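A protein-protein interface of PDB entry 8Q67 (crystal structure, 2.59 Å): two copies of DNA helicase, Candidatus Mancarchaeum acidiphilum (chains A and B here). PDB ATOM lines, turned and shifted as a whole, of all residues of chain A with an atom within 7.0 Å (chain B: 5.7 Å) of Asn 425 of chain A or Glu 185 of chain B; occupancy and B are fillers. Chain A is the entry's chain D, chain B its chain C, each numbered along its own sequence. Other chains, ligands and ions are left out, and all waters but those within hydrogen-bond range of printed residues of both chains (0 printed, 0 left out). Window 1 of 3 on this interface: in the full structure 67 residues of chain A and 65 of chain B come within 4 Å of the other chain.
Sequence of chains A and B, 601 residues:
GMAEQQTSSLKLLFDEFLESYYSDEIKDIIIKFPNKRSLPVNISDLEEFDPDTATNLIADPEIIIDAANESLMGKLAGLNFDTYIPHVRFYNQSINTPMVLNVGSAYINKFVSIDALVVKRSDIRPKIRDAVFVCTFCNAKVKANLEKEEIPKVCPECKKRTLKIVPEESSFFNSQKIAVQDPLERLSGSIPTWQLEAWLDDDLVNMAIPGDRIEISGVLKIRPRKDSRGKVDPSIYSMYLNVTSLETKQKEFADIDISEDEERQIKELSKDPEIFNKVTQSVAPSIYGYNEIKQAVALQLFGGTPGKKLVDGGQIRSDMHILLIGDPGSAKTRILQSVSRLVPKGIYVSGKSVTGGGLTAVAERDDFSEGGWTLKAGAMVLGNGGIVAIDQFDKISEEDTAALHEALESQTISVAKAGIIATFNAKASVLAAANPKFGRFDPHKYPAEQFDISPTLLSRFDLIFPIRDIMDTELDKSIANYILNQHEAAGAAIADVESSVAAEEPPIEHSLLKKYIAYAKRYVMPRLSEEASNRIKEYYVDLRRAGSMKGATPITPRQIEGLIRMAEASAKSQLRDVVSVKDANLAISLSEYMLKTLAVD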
ATOM      1  N   MET A 380      28.898  15.937  -7.314  1.00  0.00           N
ATOM      2  CA  MET A 380      29.502  15.568  -8.590  1.00  0.00           C
ATOM      3  C   MET A 380      28.786  16.244  -9.754  1.00  0.00           C
ATOM      4  O   MET A 380      29.430  16.672 -10.720  1.00  0.00           O
ATOM      5  CB  MET A 380      29.489  14.047  -8.753  1.00  0.00           C
ATOM      6  CG  MET A 380      30.476  13.305  -7.844  1.00  0.00           C
ATOM      7  SD  MET A 380      32.150  13.988  -7.839  1.00  0.00           S
ATOM      8  CE  MET A 380      32.662  13.680  -9.527  1.00  0.00           C
ATOM      9  N   VAL A 381      27.466  16.384  -9.652  1.00  0.00           N
ATOM     10  CA  VAL A 381      26.693  17.021 -10.717  1.00  0.00           C
ATOM     11  C   VAL A 381      26.606  18.545 -10.542  1.00  0.00           C
ATOM     12  O   VAL A 381      26.491  19.277 -11.524  1.00  0.00           O
ATOM     13  CB  VAL A 381      25.282  16.400 -10.855  1.00  0.00           C
ATOM     14  CG1 VAL A 381      25.388  14.897 -11.067  1.00  0.00           C
ATOM     15  CG2 VAL A 381      24.414  16.704  -9.642  1.00  0.00           C
ATOM     16  N   LEU A 382      26.660  19.017  -9.296  1.00  0.00           N
ATOM     17  CA  LEU A 382      26.610  20.453  -9.009  1.00  0.00           C
ATOM     18  C   LEU A 382      27.946  21.140  -9.192  1.00  0.00           C
ATOM     19  O   LEU A 382      28.018  22.368  -9.240  1.00  0.00           O
ATOM     20  CB  LEU A 382      26.189  20.702  -7.583  1.00  0.00           C
ATOM     21  CG  LEU A 382      24.718  20.899  -7.317  1.00  0.00           C
ATOM     22  CD1 LEU A 382      24.552  20.839  -5.808  1.00  0.00           C
ATOM     23  CD2 LEU A 382      24.340  22.241  -7.919  1.00  0.00           C
ATOM     24  N   GLY A 383      29.012  20.350  -9.292  1.00  0.00           N
ATOM     25  CA  GLY A 383      30.340  20.891  -9.482  1.00  0.00           C
ATOM     26  C   GLY A 383      30.875  20.712 -10.890  1.00  0.00           C
ATOM     27  O   GLY A 383      32.082  20.523 -11.057  1.00  0.00           O
ATOM     28  N   ASN A 384      29.996  20.735 -11.894  1.00  0.00           N
ATOM     29  CA  ASN A 384      30.446  20.617 -13.274  1.00  0.00           C
ATOM     30  C   ASN A 384      31.460  21.724 -13.546  1.00  0.00           C
ATOM     31  O   ASN A 384      31.113  22.911 -13.534  1.00  0.00           O
ATOM     32  CB  ASN A 384      29.334  20.704 -14.319  1.00  0.00           C
ATOM     33  CG  ASN A 384      28.412  19.550 -14.271  1.00  0.00           C
ATOM     34  OD1 ASN A 384      28.672  18.621 -13.538  1.00  0.00           O
ATOM     35  ND2 ASN A 384      27.555  19.448 -15.291  1.00  0.00           N
ATOM     36  N   GLN A 411      32.858  10.753 -16.273  1.00  0.00           N
ATOM     37  CA  GLN A 411      32.346  12.084 -15.953  1.00  0.00           C
ATOM     38  C   GLN A 411      30.877  12.184 -16.360  1.00  0.00           C
ATOM     39  O   GLN A 411      30.387  13.228 -16.798  1.00  0.00           O
ATOM     40  CB  GLN A 411      33.213  13.154 -16.615  1.00  0.00           C
ATOM     41  CG  GLN A 411      34.672  13.059 -16.150  1.00  0.00           C
ATOM     42  CD  GLN A 411      35.459  14.330 -16.362  1.00  0.00           C
ATOM     43  OE1 GLN A 411      35.755  14.711 -17.495  1.00  0.00           O
ATOM     44  NE2 GLN A 411      35.812  14.995 -15.265  1.00  0.00           N
ATOM     45  N   THR A 412      30.171  11.065 -16.204  1.00  0.00           N
ATOM     46  CA  THR A 412      28.740  10.970 -16.431  1.00  0.00           C
ATOM     47  C   THR A 412      28.144  10.078 -15.351  1.00  0.00           C
ATOM     48  O   THR A 412      28.796   9.137 -14.887  1.00  0.00           O
ATOM     49  CB  THR A 412      28.426  10.383 -17.806  1.00  0.00           C
ATOM     50  OG1 THR A 412      29.203   9.194 -17.994  1.00  0.00           O
ATOM     51  CG2 THR A 412      28.757  11.387 -18.903  1.00  0.00           C
ATOM     52  N   ILE A 413      26.907  10.378 -14.960  1.00  0.00           N
ATOM     53  CA  ILE A 413      26.134   9.537 -14.047  1.00  0.00           C
ATOM     54  C   ILE A 413      24.900   9.083 -14.820  1.00  0.00           C
ATOM     55  O   ILE A 413      23.972   9.870 -15.035  1.00  0.00           O
ATOM     56  CB  ILE A 413      25.746  10.266 -12.756  1.00  0.00           C
ATOM     57  CG1 ILE A 413      27.008  10.699 -12.014  1.00  0.00           C
ATOM     58  CG2 ILE A 413      24.891   9.358 -11.887  1.00  0.00           C
ATOM     59  CD1 ILE A 413      26.771  11.556 -10.799  1.00  0.00           C
ATOM     60  N   ILE A 421      15.715   7.308 -19.527  1.00  0.00           N
ATOM     61  CA  ILE A 421      17.038   6.834 -19.688  1.00  0.00           C
ATOM     62  C   ILE A 421      17.796   8.117 -19.809  1.00  0.00           C
ATOM     63  O   ILE A 421      17.589   8.837 -20.725  1.00  0.00           O
ATOM     64  CB  ILE A 421      17.158   6.124 -21.001  1.00  0.00           C
ATOM     65  CG1 ILE A 421      16.468   4.804 -20.947  1.00  0.00           C
ATOM     66  CG2 ILE A 421      18.585   5.859 -21.311  1.00  0.00           C
ATOM     67  CD1 ILE A 421      16.141   4.295 -22.305  1.00  0.00           C
ATOM     68  N   ALA A 422      18.713   8.391 -18.923  1.00  0.00           N
ATOM     69  CA  ALA A 422      19.361   9.697 -18.913  1.00  0.00           C
ATOM     70  C   ALA A 422      20.811   9.612 -18.470  1.00  0.00           C
ATOM     71  O   ALA A 422      21.147   8.875 -17.543  1.00  0.00           O
ATOM     72  CB  ALA A 422      18.616  10.681 -17.998  1.00  0.00           C
ATOM     73  N   THR A 423      21.659  10.409 -19.114  1.00  0.00           N
ATOM     74  CA  THR A 423      23.088  10.473 -18.814  1.00  0.00           C
ATOM     75  C   THR A 423      23.399  11.864 -18.255  1.00  0.00           C
ATOM     76  O   THR A 423      23.668  12.806 -19.004  1.00  0.00           O
ATOM     77  CB  THR A 423      23.913  10.172 -20.067  1.00  0.00           C
ATOM     78  OG1 THR A 423      23.467   8.949 -20.667  1.00  0.00           O
ATOM     79  CG2 THR A 423      25.381  10.036 -19.718  1.00  0.00           C
ATOM     80  N   PHE A 424      23.349  11.990 -16.929  1.00  0.00           N
ATOM     81  CA  PHE A 424      23.690  13.243 -16.272  1.00  0.00           C
ATOM     82  C   PHE A 424      25.167  13.566 -16.469  1.00  0.00           C
ATOM     83  O   PHE A 424      26.013  12.672 -16.540  1.00  0.00           O
ATOM     84  CB  PHE A 424      23.397  13.153 -14.771  1.00  0.00           C
ATOM     85  CG  PHE A 424      21.936  13.244 -14.423  1.00  0.00           C
ATOM     86  CD1 PHE A 424      21.120  12.120 -14.461  1.00  0.00           C
ATOM     87  CD2 PHE A 424      21.379  14.457 -14.054  1.00  0.00           C
ATOM     88  CE1 PHE A 424      19.773  12.211 -14.140  1.00  0.00           C
ATOM     89  CE2 PHE A 424      20.036  14.554 -13.731  1.00  0.00           C
ATOM     90  CZ  PHE A 424      19.232  13.430 -13.776  1.00  0.00           C
ATOM     91  N   ASN A 425      25.481  14.859 -16.495  1.00  0.00           N
ATOM     92  CA  ASN A 425      26.860  15.318 -16.610  1.00  0.00           C
ATOM     93  C   ASN A 425      27.463  15.534 -15.225  1.00  0.00           C
ATOM     94  O   ASN A 425      26.900  16.258 -14.399  1.00  0.00           O
ATOM     95  CB  ASN A 425      26.926  16.613 -17.418  1.00  0.00           C
ATOM     96  CG  ASN A 425      26.462  16.428 -18.849  1.00  0.00           C
ATOM     97  OD1 ASN A 425      26.647  15.365 -19.440  1.00  0.00           O
ATOM     98  ND2 ASN A 425      25.850  17.465 -19.412  1.00  0.00           N
ATOM     99  N   ALA A 426      28.613  14.918 -14.983  1.00  0.00           N
ATOM    100  CA  ALA A 426      29.294  15.009 -13.699  1.00  0.00           C
ATOM    101  C   ALA A 426      30.776  15.273 -13.923  1.00  0.00           C
ATOM    102  O   ALA A 426      31.646  14.591 -13.383  1.00  0.00           O
ATOM    103  CB  ALA A 426      29.088  13.736 -12.876  1.00  0.00           C
ATOM    104  N   LYS A 427      31.099  16.240 -14.765  1.00  0.00           N
ATOM    105  CA  LYS A 427      32.500  16.585 -14.948  1.00  0.00           C
ATOM    106  C   LYS A 427      33.072  17.353 -13.771  1.00  0.00           C
ATOM    107  O   LYS A 427      32.589  18.437 -13.430  1.00  0.00           O
ATOM    108  CB  LYS A 427      32.717  17.393 -16.218  1.00  0.00           C
ATOM    109  CG  LYS A 427      34.119  17.999 -16.205  1.00  0.00           C
ATOM    110  CD  LYS A 427      34.522  18.406 -17.599  1.00  0.00           C
ATOM    111  CE  LYS A 427      35.970  18.823 -17.732  1.00  0.00           C
ATOM    112  NZ  LYS A 427      36.750  17.516 -17.635  1.00  0.00           N
ATOM    113  N   PRO B 183      16.959  17.409 -23.125  1.00  0.00           N
ATOM    114  CA  PRO B 183      17.609  16.187 -22.650  1.00  0.00           C
ATOM    115  C   PRO B 183      18.532  16.506 -21.485  1.00  0.00           C
ATOM    116  O   PRO B 183      19.182  17.554 -21.443  1.00  0.00           O
ATOM    117  CB  PRO B 183      18.382  15.699 -23.879  1.00  0.00           C
ATOM    118  CG  PRO B 183      17.502  16.153 -25.031  1.00  0.00           C
ATOM    119  CD  PRO B 183      17.039  17.532 -24.595  1.00  0.00           C
ATOM    120  N   LEU B 184      18.572  15.580 -20.523  1.00  0.00           N
ATOM    121  CA  LEU B 184      19.424  15.755 -19.355  1.00  0.00           C
ATOM    122  C   LEU B 184      20.887  15.881 -19.750  1.00  0.00           C
ATOM    123  O   LEU B 184      21.686  16.403 -18.964  1.00  0.00           O
ATOM    124  CB  LEU B 184      19.254  14.579 -18.384  1.00  0.00           C
ATOM    125  CG  LEU B 184      18.036  14.615 -17.453  1.00  0.00           C
ATOM    126  CD1 LEU B 184      18.049  15.805 -16.493  1.00  0.00           C
ATOM    127  CD2 LEU B 184      16.756  14.579 -18.288  1.00  0.00           C
ATOM    128  N   GLU B 185      21.262  15.413 -20.945  1.00  0.00           N
ATOM    129  CA  GLU B 185      22.666  15.429 -21.329  1.00  0.00           C
ATOM    130  C   GLU B 185      23.117  16.811 -21.786  1.00  0.00           C
ATOM    131  O   GLU B 185      24.319  17.092 -21.766  1.00  0.00           O
ATOM    132  CB  GLU B 185      22.936  14.417 -22.450  1.00  0.00           C
ATOM    133  CG  GLU B 185      22.504  13.004 -22.075  1.00  0.00           C
ATOM    134  CD  GLU B 185      21.063  12.691 -22.525  1.00  0.00           C
ATOM    135  OE1 GLU B 185      20.490  13.449 -23.350  1.00  0.00           O
ATOM    136  OE2 GLU B 185      20.455  11.745 -21.963  1.00  0.00           O
ATOM    137  N   ARG B 186      22.180  17.667 -22.203  1.00  0.00           N
ATOM    138  CA  ARG B 186      22.480  19.016 -22.665  1.00  0.00           C
ATOM    139  C   ARG B 186      22.528  20.043 -21.536  1.00  0.00           C
ATOM    140  O   ARG B 186      22.961  21.175 -21.771  1.00  0.00           O
ATOM    141  CB  ARG B 186      21.432  19.452 -23.699  1.00  0.00           C
ATOM    142  CG  ARG B 186      21.405  18.583 -24.951  1.00  0.00           C
ATOM    143  CD  ARG B 186      20.647  19.242 -26.086  1.00  0.00           C
ATOM    144  NE  ARG B 186      21.337  20.430 -26.579  1.00  0.00           N
ATOM    145  CZ  ARG B 186      20.760  21.366 -27.323  1.00  0.00           C
ATOM    146  NH1 ARG B 186      19.484  21.246 -27.660  1.00  0.00           N
ATOM    147  NH2 ARG B 186      21.454  22.419 -27.730  1.00  0.00           N
ATOM    148  N   LEU B 187      22.100  19.687 -20.327  1.00  0.00           N
ATOM    149  CA  LEU B 187      22.098  20.616 -19.203  1.00  0.00           C
ATOM    150  C   LEU B 187      23.437  20.569 -18.475  1.00  0.00           C
ATOM    151  O   LEU B 187      24.049  19.505 -18.346  1.00  0.00           O
ATOM    152  CB  LEU B 187      20.962  20.273 -18.238  1.00  0.00           C
ATOM    153  CG  LEU B 187      19.555  20.310 -18.840  1.00  0.00           C
ATOM    154  CD1 LEU B 187      18.549  19.707 -17.871  1.00  0.00           C
ATOM    155  CD2 LEU B 187      19.174  21.735 -19.210  1.00  0.00           C
ATOM    156  N   SER B 188      23.889  21.733 -18.005  1.00  0.00           N
ATOM    157  CA  SER B 188      25.166  21.849 -17.310  1.00  0.00           C
ATOM    158  C   SER B 188      25.034  21.810 -15.793  1.00  0.00           C
ATOM    159  O   SER B 188      26.056  21.751 -15.102  1.00  0.00           O
ATOM    160  CB  SER B 188      25.865  23.154 -17.713  1.00  0.00           C
ATOM    161  OG  SER B 188      25.097  24.277 -17.313  1.00  0.00           O
ATOM    162  N   ARG B 213      13.441  10.868 -27.336  1.00  0.00           N
ATOM    163  CA  ARG B 213      14.155  12.103 -27.656  1.00  0.00           C
ATOM    164  C   ARG B 213      13.910  12.377 -29.134  1.00  0.00           C
ATOM    165  O   ARG B 213      14.400  11.642 -29.998  1.00  0.00           O
ATOM    166  CB  ARG B 213      15.646  11.993 -27.347  1.00  0.00           C
ATOM    167  CG  ARG B 213      16.436  13.256 -27.672  1.00  0.00           C
ATOM    168  CD  ARG B 213      17.826  13.209 -27.057  1.00  0.00           C
ATOM    169  NE  ARG B 213      18.729  14.204 -27.629  1.00  0.00           N
ATOM    170  CZ  ARG B 213      19.966  14.426 -27.196  1.00  0.00           C
ATOM    171  NH1 ARG B 213      20.448  13.727 -26.175  1.00  0.00           N
ATOM    172  NH2 ARG B 213      20.722  15.344 -27.782  1.00  0.00           N
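Among the printed residues, pairs that only touch across the chains: Ala 422 of chain A with Leu 184 of chain B (3.97 Å), Ala 422 of chain A with Glu 185 of chain B (3.8 Å) and Phe 424 of chain A with Leu 184 of chain B (3.6 Å).
The guanidinium group of Arg 213 of chain B lies within salt-bridge range of the side-chain carboxylate of Glu 185 of chain B (2.8 Å).
OD1 of Asn 384 of chain A lies close to O of Val 381 of chain A, at 3.0 Å.
The backbone carbonyl oxygen (O) of Asn 425 of chain A lies close to the side-chain amide oxygen (OD1) of Asn 384 of chain A, at 3.1 Å.
The backbone carbonyl oxygen of Ile 413 of chain A is in hydrogen-bond range of the backbone NH of Phe 424 of chain A (2.9 Å).
Of the 7 printed residues of chain B, 4 touch a printed residue of chain A.
Hydrophobic or aromatic side chains of chain B that line the printed part of chain A: Leu 184.
Among the printed residues, 7 pairs touch across the chains.
Among the printed residues, no Asp or Glu carboxylate lies within 4 Å of a Lys or Arg side-chain nitrogen of the other chain.
The side-chain carboxylate (OE2) of Glu 185 of chain B lies within hydrogen-bond range of the backbone NH (N) of Thr 423 of chain A (3.4 Å).
The backbone carbonyl oxygen (O) of Glu 185 of chain B sits at hydrogen-bond distance from the side-chain amide nitrogen (ND2) of Asn 425 of chain A.
ND2 of Asn 425 of chain A is in hydrogen-bond range of O of Leu 187 of chain B, 2.9 Å away.
The side-chain amide nitrogen of Asn 384 of chain A sits at hydrogen-bond distance from the backbone carbonyl oxygen of Ser 188 of chain B (2.8 Å).
Asn 425 of chain A touches just these residues of chain B: Glu 185 (2.8 Å) and Leu 187 (2.9 Å).
Of chain A, only Ala 422 (3.8 Å), Thr 423 (3.3 Å) and Asn 425 (2.8 Å) come within 4 Å of Glu 185 of chain B.
Of the printed residues of chain B, Thr 423 of chain A touches Glu 185.
Of the printed residues of chain B, Phe 424 of chain A touches Leu 184 (3.6 Å).
Leu 382 of chain A touches none of the printed residues of chain B.
The nearest residue of chain B that does not touch Asn 425 of chain A is Leu 184 of chain B (4.3 Å).
The nearest residue of chain A that does not touch Glu 185 of chain B is Ile 421 of chain A (4.3 Å).
The nearest printed residue of chain B that does not touch Ala 422 of chain A is Pro 183 of chain B (6.8 Å).
No position is printed for both chains.
Of the 7 pairs that touch across the chains among the printed residues, none has its exchanged pair printed and touching as well.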
